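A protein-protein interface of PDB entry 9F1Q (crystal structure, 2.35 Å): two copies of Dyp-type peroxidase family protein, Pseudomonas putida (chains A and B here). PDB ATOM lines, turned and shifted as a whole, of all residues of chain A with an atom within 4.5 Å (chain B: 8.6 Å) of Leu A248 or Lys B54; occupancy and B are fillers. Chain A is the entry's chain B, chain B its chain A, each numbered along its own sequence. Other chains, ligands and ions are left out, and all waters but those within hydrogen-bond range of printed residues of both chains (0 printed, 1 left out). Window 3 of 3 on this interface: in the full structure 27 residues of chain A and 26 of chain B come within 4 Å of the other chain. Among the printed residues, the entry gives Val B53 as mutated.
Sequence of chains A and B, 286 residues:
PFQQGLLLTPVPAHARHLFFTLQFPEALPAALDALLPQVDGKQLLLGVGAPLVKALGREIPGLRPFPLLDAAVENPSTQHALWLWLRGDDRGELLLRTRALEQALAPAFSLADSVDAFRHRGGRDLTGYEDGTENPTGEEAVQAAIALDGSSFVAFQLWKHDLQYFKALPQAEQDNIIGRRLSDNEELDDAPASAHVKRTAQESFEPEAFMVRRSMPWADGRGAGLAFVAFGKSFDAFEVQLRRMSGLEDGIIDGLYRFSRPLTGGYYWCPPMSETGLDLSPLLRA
Ala A71 touches just these residues of chain B: Pro B51 (3.5 Å) and Lys B54 (3.9 Å). Of the printed residues of chain B, Ala A72 touches Pro B51, Lys B54 and Ala B55. Leu A248 touches one residue of chain B. Of the printed residues of chain A, Ala B50 touches Asp A70. Printed residues of chain A within 4 Å of Pro B51: Ala A71 (3.5 Å) and Ala A72 (3.8 Å). Lys B54 touches just these residues of chain A: Asp A70 (3.7 Å), Ala A71 (3.9 Å), Ala A72 (3.9 Å) and Leu A248 (3.9 Å). Printed residues of chain A within 4 Å of Ala B55: Ala A72 (3.8 Å). Printed residues of chain A within 4 Å of Pro B65: Asp A70. The nearest printed residue of chain B that does not touch Leu A248 is Pro B65 (9.4 Å). The nearest printed residue of chain A that does not touch Lys B54 is Gly A247 (5.1 Å).
Printed residues of chain A that touch a printed residue of chain B: Asp A70, Ala A71, Ala A72 and Leu A248. Among the printed residues, no Asp or Glu carboxylate lies within 4 Å of a Lys or Arg side-chain nitrogen of the other chain.
The backbone carbonyl oxygen of Arg A243 lies within hydrogen-bond range of the backbone NH of Leu A248 (2.9 Å).
No position is printed for both chains. Of the 9 pairs that touch across the chains among the printed residues, none has its exchanged pair printed and touching as well.
Asp A70 touches Ala B50. Asp A70 touches Lys B54 (O to CE, 3.7 Å). Pro B65 touches Asp A70. Ala A71 touches Pro B51. Ala A71 touches Lys B54. Ala A72 touches Pro B51 (CA to O, 3.8 Å). Lys B54 touches Ala A72 (CB to N, 3.9 Å). CA of Ala B55 touches CB of Ala A72, 3.8 Å away. Leu A248 touches Lys B54 (CD2 to NZ, 3.9 Å).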
ATOM      1  N   LEU A  69     -27.341 -12.131 -20.314  1.00  0.00           N
ATOM      2  CA  LEU A  69     -26.495 -13.223 -20.777  1.00  0.00           C
ATOM      3  C   LEU A  69     -25.393 -12.668 -21.673  1.00  0.00           C
ATOM      4  O   LEU A  69     -25.679 -12.079 -22.721  1.00  0.00           O
ATOM      5  CB  LEU A  69     -27.315 -14.276 -21.523  1.00  0.00           C
ATOM      6  CG  LEU A  69     -27.965 -15.398 -20.703  1.00  0.00           C
ATOM      7  CD1 LEU A  69     -28.930 -14.853 -19.660  1.00  0.00           C
ATOM      8  CD2 LEU A  69     -28.669 -16.388 -21.617  1.00  0.00           C
ATOM      9  N   ASP A  70     -24.139 -12.862 -21.260  1.00  0.00           N
ATOM     10  CA  ASP A  70     -22.976 -12.400 -22.018  1.00  0.00           C
ATOM     11  C   ASP A  70     -22.535 -13.519 -22.959  1.00  0.00           C
ATOM     12  O   ASP A  70     -21.577 -14.252 -22.705  1.00  0.00           O
ATOM     13  CB  ASP A  70     -21.860 -11.979 -21.069  1.00  0.00           C
ATOM     14  CG  ASP A  70     -20.686 -11.343 -21.791  1.00  0.00           C
ATOM     15  OD1 ASP A  70     -20.760 -11.158 -23.025  1.00  0.00           O
ATOM     16  OD2 ASP A  70     -19.680 -11.030 -21.120  1.00  0.00           O
ATOM     17  N   ALA A  71     -23.247 -13.639 -24.077  1.00  0.00           N
ATOM     18  CA  ALA A  71     -23.063 -14.742 -25.011  1.00  0.00           C
ATOM     19  C   ALA A  71     -22.822 -14.199 -26.415  1.00  0.00           C
ATOM     20  O   ALA A  71     -22.861 -12.987 -26.656  1.00  0.00           O
ATOM     21  CB  ALA A  71     -24.274 -15.684 -24.995  1.00  0.00           C
ATOM     22  N   ALA A  72     -22.570 -15.116 -27.351  1.00  0.00           N
ATOM     23  CA  ALA A  72     -22.377 -14.753 -28.748  1.00  0.00           C
ATOM     24  C   ALA A  72     -23.688 -14.508 -29.479  1.00  0.00           C
ATOM     25  O   ALA A  72     -23.664 -14.070 -30.634  1.00  0.00           O
ATOM     26  CB  ALA A  72     -21.581 -15.843 -29.472  1.00  0.00           C
ATOM     27  N   ARG A 243     -29.406 -20.386 -20.923  1.00  0.00           N
ATOM     28  CA  ARG A 243     -27.951 -20.294 -20.897  1.00  0.00           C
ATOM     29  C   ARG A 243     -27.309 -21.420 -21.696  1.00  0.00           C
ATOM     30  O   ARG A 243     -26.254 -21.216 -22.307  1.00  0.00           O
ATOM     31  CB  ARG A 243     -27.442 -20.277 -19.456  1.00  0.00           C
ATOM     32  CG  ARG A 243     -27.914 -19.053 -18.676  1.00  0.00           C
ATOM     33  CD  ARG A 243     -27.257 -18.914 -17.309  1.00  0.00           C
ATOM     34  NE  ARG A 243     -25.850 -18.541 -17.405  1.00  0.00           N
ATOM     35  CZ  ARG A 243     -24.832 -19.383 -17.297  1.00  0.00           C
ATOM     36  NH1 ARG A 243     -25.023 -20.677 -17.099  1.00  0.00           N
ATOM     37  NH2 ARG A 243     -23.590 -18.915 -17.393  1.00  0.00           N
ATOM     38  N   SER A 246     -27.750 -20.559 -25.393  1.00  0.00           N
ATOM     39  CA  SER A 246     -26.852 -19.482 -25.788  1.00  0.00           C
ATOM     40  C   SER A 246     -25.386 -19.902 -25.825  1.00  0.00           C
ATOM     41  O   SER A 246     -24.523 -19.049 -26.057  1.00  0.00           O
ATOM     42  CB  SER A 246     -27.027 -18.288 -24.844  1.00  0.00           C
ATOM     43  OG  SER A 246     -28.374 -17.845 -24.838  1.00  0.00           O
ATOM     44  N   GLY A 247     -25.081 -21.177 -25.599  1.00  0.00           N
ATOM     45  CA  GLY A 247     -23.710 -21.640 -25.644  1.00  0.00           C
ATOM     46  C   GLY A 247     -22.882 -21.346 -24.414  1.00  0.00           C
ATOM     47  O   GLY A 247     -21.657 -21.501 -24.463  1.00  0.00           O
ATOM     48  N   LEU A 248     -23.501 -20.925 -23.314  1.00  0.00           N
ATOM     49  CA  LEU A 248     -22.762 -20.590 -22.105  1.00  0.00           C
ATOM     50  C   LEU A 248     -22.478 -21.798 -21.224  1.00  0.00           C
ATOM     51  O   LEU A 248     -21.738 -21.667 -20.242  1.00  0.00           O
ATOM     52  CB  LEU A 248     -23.520 -19.535 -21.295  1.00  0.00           C
ATOM     53  CG  LEU A 248     -23.688 -18.182 -21.986  1.00  0.00           C
ATOM     54  CD1 LEU A 248     -24.452 -17.216 -21.096  1.00  0.00           C
ATOM     55  CD2 LEU A 248     -22.329 -17.614 -22.366  1.00  0.00           C
ATOM     56  N   GLU A 249     -23.038 -22.963 -21.545  1.00  0.00           N
ATOM     57  CA  GLU A 249     -22.780 -24.170 -20.770  1.00  0.00           C
ATOM     58  C   GLU A 249     -21.641 -24.990 -21.365  1.00  0.00           C
ATOM     59  O   GLU A 249     -20.720 -25.392 -20.647  1.00  0.00           O
ATOM     60  CB  GLU A 249     -24.053 -25.017 -20.676  1.00  0.00           C
ATOM     61  CG  GLU A 249     -24.079 -25.977 -19.495  1.00  0.00           C
ATOM     62  CD  GLU A 249     -25.294 -26.882 -19.508  1.00  0.00           C
ATOM     63  OE1 GLU A 249     -25.671 -27.356 -20.599  1.00  0.00           O
ATOM     64  OE2 GLU A 249     -25.885 -27.108 -18.430  1.00  0.00           O
ATOM     65  N   ASP A 250     -21.687 -25.244 -22.678  1.00  0.00           N
ATOM     66  CA  ASP A 250     -20.684 -26.086 -23.316  1.00  0.00           C
ATOM     67  C   ASP A 250     -20.193 -25.516 -24.644  1.00  0.00           C
ATOM     68  O   ASP A 250     -19.569 -26.243 -25.425  1.00  0.00           O
ATOM     69  CB  ASP A 250     -21.230 -27.500 -23.539  1.00  0.00           C
ATOM     70  CG  ASP A 250     -22.552 -27.507 -24.295  1.00  0.00           C
ATOM     71  OD1 ASP A 250     -22.925 -26.463 -24.872  1.00  0.00           O
ATOM     72  OD2 ASP A 250     -23.216 -28.562 -24.318  1.00  0.00           O
ATOM     73  N   LEU B  22     -24.788  -9.933 -35.432  1.00  0.00           N
ATOM     74  CA  LEU B  22     -23.945 -10.903 -36.126  1.00  0.00           C
ATOM     75  C   LEU B  22     -24.790 -12.151 -36.336  1.00  0.00           C
ATOM     76  O   LEU B  22     -24.874 -13.030 -35.477  1.00  0.00           O
ATOM     77  CB  LEU B  22     -22.677 -11.199 -35.340  1.00  0.00           C
ATOM     78  CG  LEU B  22     -21.684 -12.092 -36.086  1.00  0.00           C
ATOM     79  CD1 LEU B  22     -21.263 -11.444 -37.401  1.00  0.00           C
ATOM     80  CD2 LEU B  22     -20.475 -12.385 -35.221  1.00  0.00           C
ATOM     81  N   PRO B  25     -21.812 -15.647 -38.256  1.00  0.00           N
ATOM     82  CA  PRO B  25     -20.418 -15.292 -37.941  1.00  0.00           C
ATOM     83  C   PRO B  25     -19.397 -15.917 -38.873  1.00  0.00           C
ATOM     84  O   PRO B  25     -18.282 -15.393 -38.977  1.00  0.00           O
ATOM     85  CB  PRO B  25     -20.241 -15.787 -36.499  1.00  0.00           C
ATOM     86  CG  PRO B  25     -21.321 -16.796 -36.291  1.00  0.00           C
ATOM     87  CD  PRO B  25     -22.464 -16.395 -37.168  1.00  0.00           C
ATOM     88  N   VAL B  48     -17.526  -1.934 -31.330  1.00  0.00           N
ATOM     89  CA  VAL B  48     -17.596  -3.391 -31.281  1.00  0.00           C
ATOM     90  C   VAL B  48     -18.326  -3.794 -30.008  1.00  0.00           C
ATOM     91  O   VAL B  48     -17.993  -3.318 -28.916  1.00  0.00           O
ATOM     92  CB  VAL B  48     -16.197  -4.029 -31.338  1.00  0.00           C
ATOM     93  CG1 VAL B  48     -16.299  -5.539 -31.184  1.00  0.00           C
ATOM     94  CG2 VAL B  48     -15.496  -3.671 -32.640  1.00  0.00           C
ATOM     95  N   GLY B  49     -19.318  -4.671 -30.146  1.00  0.00           N
ATOM     96  CA  GLY B  49     -20.092  -5.134 -29.018  1.00  0.00           C
ATOM     97  C   GLY B  49     -19.615  -6.473 -28.487  1.00  0.00           C
ATOM     98  O   GLY B  49     -18.939  -7.234 -29.175  1.00  0.00           O
ATOM     99  N   ALA B  50     -19.989  -6.746 -27.236  1.00  0.00           N
ATOM    100  CA  ALA B  50     -19.587  -7.995 -26.592  1.00  0.00           C
ATOM    101  C   ALA B  50     -20.003  -9.254 -27.351  1.00  0.00           C
ATOM    102  O   ALA B  50     -19.222 -10.220 -27.345  1.00  0.00           O
ATOM    103  CB  ALA B  50     -20.129  -8.027 -25.157  1.00  0.00           C
ATOM    104  N   PRO B  51     -21.183  -9.336 -27.986  1.00  0.00           N
ATOM    105  CA  PRO B  51     -21.494 -10.562 -28.745  1.00  0.00           C
ATOM    106  C   PRO B  51     -20.507 -10.847 -29.863  1.00  0.00           C
ATOM    107  O   PRO B  51     -20.171 -12.013 -30.104  1.00  0.00           O
ATOM    108  CB  PRO B  51     -22.904 -10.286 -29.285  1.00  0.00           C
ATOM    109  CG  PRO B  51     -23.494  -9.349 -28.304  1.00  0.00           C
ATOM    110  CD  PRO B  51     -22.367  -8.461 -27.873  1.00  0.00           C
ATOM    111  N   LEU B  52     -20.040  -9.811 -30.562  1.00  0.00           N
ATOM    112  CA  LEU B  52     -19.060 -10.016 -31.623  1.00  0.00           C
ATOM    113  C   LEU B  52     -17.749 -10.563 -31.065  1.00  0.00           C
ATOM    114  O   LEU B  52     -17.134 -11.453 -31.664  1.00  0.00           O
ATOM    115  CB  LEU B  52     -18.825  -8.708 -32.380  1.00  0.00           C
ATOM    116  CG  LEU B  52     -17.752  -8.725 -33.471  1.00  0.00           C
ATOM    117  CD1 LEU B  52     -18.007  -9.835 -34.475  1.00  0.00           C
ATOM    118  CD2 LEU B  52     -17.697  -7.381 -34.173  1.00  0.00           C
ATOM    119  N   VAL B  53     -17.304 -10.036 -29.923  1.00  0.00           N
ATOM    120  CA  VAL B  53     -16.071 -10.524 -29.310  1.00  0.00           C
ATOM    121  C   VAL B  53     -16.234 -11.969 -28.849  1.00  0.00           C
ATOM    122  O   VAL B  53     -15.341 -12.802 -29.049  1.00  0.00           O
ATOM    123  CB  VAL B  53     -15.657  -9.601 -28.150  1.00  0.00           C
ATOM    124  CG1 VAL B  53     -14.429 -10.149 -27.449  1.00  0.00           C
ATOM    125  CG2 VAL B  53     -15.397  -8.195 -28.662  1.00  0.00           C
ATOM    126  N   LYS B  54     -17.372 -12.287 -28.225  1.00  0.00           N
ATOM    127  CA  LYS B  54     -17.618 -13.654 -27.774  1.00  0.00           C
ATOM    128  C   LYS B  54     -17.695 -14.628 -28.942  1.00  0.00           C
ATOM    129  O   LYS B  54     -17.271 -15.783 -28.814  1.00  0.00           O
ATOM    130  CB  LYS B  54     -18.903 -13.712 -26.948  1.00  0.00           C
ATOM    131  CG  LYS B  54     -18.691 -13.554 -25.451  1.00  0.00           C
ATOM    132  CD  LYS B  54     -18.261 -14.866 -24.815  1.00  0.00           C
ATOM    133  CE  LYS B  54     -19.306 -15.951 -25.036  1.00  0.00           C
ATOM    134  NZ  LYS B  54     -18.960 -17.212 -24.325  1.00  0.00           N
ATOM    135  N   ALA B  55     -18.234 -14.188 -30.082  1.00  0.00           N
ATOM    136  CA  ALA B  55     -18.338 -15.076 -31.234  1.00  0.00           C
ATOM    137  C   ALA B  55     -16.967 -15.441 -31.786  1.00  0.00           C
ATOM    138  O   ALA B  55     -16.805 -16.516 -32.375  1.00  0.00           O
ATOM    139  CB  ALA B  55     -19.193 -14.428 -32.324  1.00  0.00           C
ATOM    140  N   LEU B  56     -15.976 -14.569 -31.612  1.00  0.00           N
ATOM    141  CA  LEU B  56     -14.606 -14.858 -32.014  1.00  0.00           C
ATOM    142  C   LEU B  56     -13.795 -15.537 -30.919  1.00  0.00           C
ATOM    143  O   LEU B  56     -12.600 -15.780 -31.114  1.00  0.00           O
ATOM    144  CB  LEU B  56     -13.901 -13.567 -32.450  1.00  0.00           C
ATOM    145  CG  LEU B  56     -14.445 -12.901 -33.714  1.00  0.00           C
ATOM    146  CD1 LEU B  56     -13.686 -11.618 -34.011  1.00  0.00           C
ATOM    147  CD2 LEU B  56     -14.378 -13.858 -34.895  1.00  0.00           C
ATOM    148  N   GLY B  57     -14.410 -15.852 -29.780  1.00  0.00           N
ATOM    149  CA  GLY B  57     -13.691 -16.478 -28.683  1.00  0.00           C
ATOM    150  C   GLY B  57     -12.559 -15.649 -28.117  1.00  0.00           C
ATOM    151  O   GLY B  57     -11.581 -16.210 -27.614  1.00  0.00           O
ATOM    152  N   ARG B  58     -12.660 -14.327 -28.192  1.00  0.00           N
ATOM    153  CA  ARG B  58     -11.634 -13.423 -27.694  1.00  0.00           C
ATOM    154  C   ARG B  58     -12.165 -12.612 -26.514  1.00  0.00           C
ATOM    155  O   ARG B  58     -13.287 -12.811 -26.041  1.00  0.00           O
ATOM    156  CB  ARG B  58     -11.122 -12.516 -28.812  1.00  0.00           C
ATOM    157  CG  ARG B  58     -10.470 -13.276 -29.953  1.00  0.00           C
ATOM    158  CD  ARG B  58      -9.744 -12.331 -30.887  1.00  0.00           C
ATOM    159  NE  ARG B  58      -8.920 -13.046 -31.855  1.00  0.00           N
ATOM    160  CZ  ARG B  58      -7.600 -13.138 -31.783  1.00  0.00           C
ATOM    161  NH1 ARG B  58      -6.919 -12.558 -30.809  1.00  0.00           N
ATOM    162  NH2 ARG B  58      -6.945 -13.830 -32.711  1.00  0.00           N
ATOM    163  N   GLU B  59     -11.335 -11.683 -26.041  1.00  0.00           N
ATOM    164  CA  GLU B  59     -11.672 -10.826 -24.913  1.00  0.00           C
ATOM    165  C   GLU B  59     -11.049  -9.455 -25.119  1.00  0.00           C
ATOM    166  O   GLU B  59      -9.898  -9.346 -25.548  1.00  0.00           O
ATOM    167  CB  GLU B  59     -11.180 -11.416 -23.584  1.00  0.00           C
ATOM    168  CG  GLU B  59     -11.923 -12.654 -23.116  1.00  0.00           C
ATOM    169  CD  GLU B  59     -11.402 -13.175 -21.792  1.00  0.00           C
ATOM    170  OE1 GLU B  59     -10.304 -12.745 -21.377  1.00  0.00           O
ATOM    171  OE2 GLU B  59     -12.074 -14.029 -21.178  1.00  0.00           O
ATOM    172  N   ILE B  60     -11.816  -8.416 -24.808  1.00  0.00           N
ATOM    173  CA  ILE B  60     -11.362  -7.035 -24.883  1.00  0.00           C
ATOM    174  C   ILE B  60     -11.387  -6.459 -23.474  1.00  0.00           C
ATOM    175  O   ILE B  60     -12.459  -6.356 -22.870  1.00  0.00           O
ATOM    176  CB  ILE B  60     -12.227  -6.187 -25.828  1.00  0.00           C
ATOM    177  CG1 ILE B  60     -12.166  -6.745 -27.251  1.00  0.00           C
ATOM    178  CG2 ILE B  60     -11.781  -4.731 -25.791  1.00  0.00           C
ATOM    179  CD1 ILE B  60     -10.785  -6.691 -27.860  1.00  0.00           C
ATOM    180  N   LEU B  63     -14.375  -4.161 -21.992  1.00  0.00           N
ATOM    181  CA  LEU B  63     -15.610  -4.353 -22.736  1.00  0.00           C
ATOM    182  C   LEU B  63     -16.509  -5.364 -22.038  1.00  0.00           C
ATOM    183  O   LEU B  63     -16.043  -6.403 -21.558  1.00  0.00           O
ATOM    184  CB  LEU B  63     -15.329  -4.818 -24.167  1.00  0.00           C
ATOM    185  CG  LEU B  63     -16.572  -4.998 -25.042  1.00  0.00           C
ATOM    186  CD1 LEU B  63     -17.384  -3.711 -25.105  1.00  0.00           C
ATOM    187  CD2 LEU B  63     -16.192  -5.459 -26.439  1.00  0.00           C
ATOM    188  N   PRO B  65     -21.205  -6.274 -21.863  1.00  0.00           N
ATOM    189  CA  PRO B  65     -22.526  -5.838 -22.332  1.00  0.00           C
ATOM    190  C   PRO B  65     -23.117  -4.756 -21.438  1.00  0.00           C
ATOM    191  O   PRO B  65     -22.684  -4.536 -20.305  1.00  0.00           O
ATOM    192  CB  PRO B  65     -23.369  -7.118 -22.289  1.00  0.00           C
ATOM    193  CG  PRO B  65     -22.652  -8.028 -21.360  1.00  0.00           C
ATOM    194  CD  PRO B  65     -21.198  -7.697 -21.477  1.00  0.00           C
ATOM    195  N   ALA B  81     -23.996  -6.451 -31.848  1.00  0.00           N
ATOM    196  CA  ALA B  81     -22.621  -6.825 -32.159  1.00  0.00           C
ATOM    197  C   ALA B  81     -21.818  -5.677 -32.755  1.00  0.00           C
ATOM    198  O   ALA B  81     -20.603  -5.609 -32.546  1.00  0.00           O
ATOM    199  CB  ALA B  81     -22.604  -8.019 -33.116  1.00  0.00           C
ATOM    200  N   LEU B 283      -8.389  -7.927 -31.982  1.00  0.00           N
ATOM    201  CA  LEU B 283      -9.482  -8.830 -32.298  1.00  0.00           C
ATOM    202  C   LEU B 283      -9.185  -9.787 -33.443  1.00  0.00           C
ATOM    203  O   LEU B 283      -9.870 -10.808 -33.557  1.00  0.00           O
ATOM    204  CB  LEU B 283     -10.747  -8.028 -32.641  1.00  0.00           C
ATOM    205  CG  LEU B 283     -12.098  -8.708 -32.415  1.00  0.00           C
ATOM    206  CD1 LEU B 283     -12.297  -9.024 -30.942  1.00  0.00           C
ATOM    207  CD2 LEU B 283     -13.226  -7.832 -32.939  1.00  0.00           C
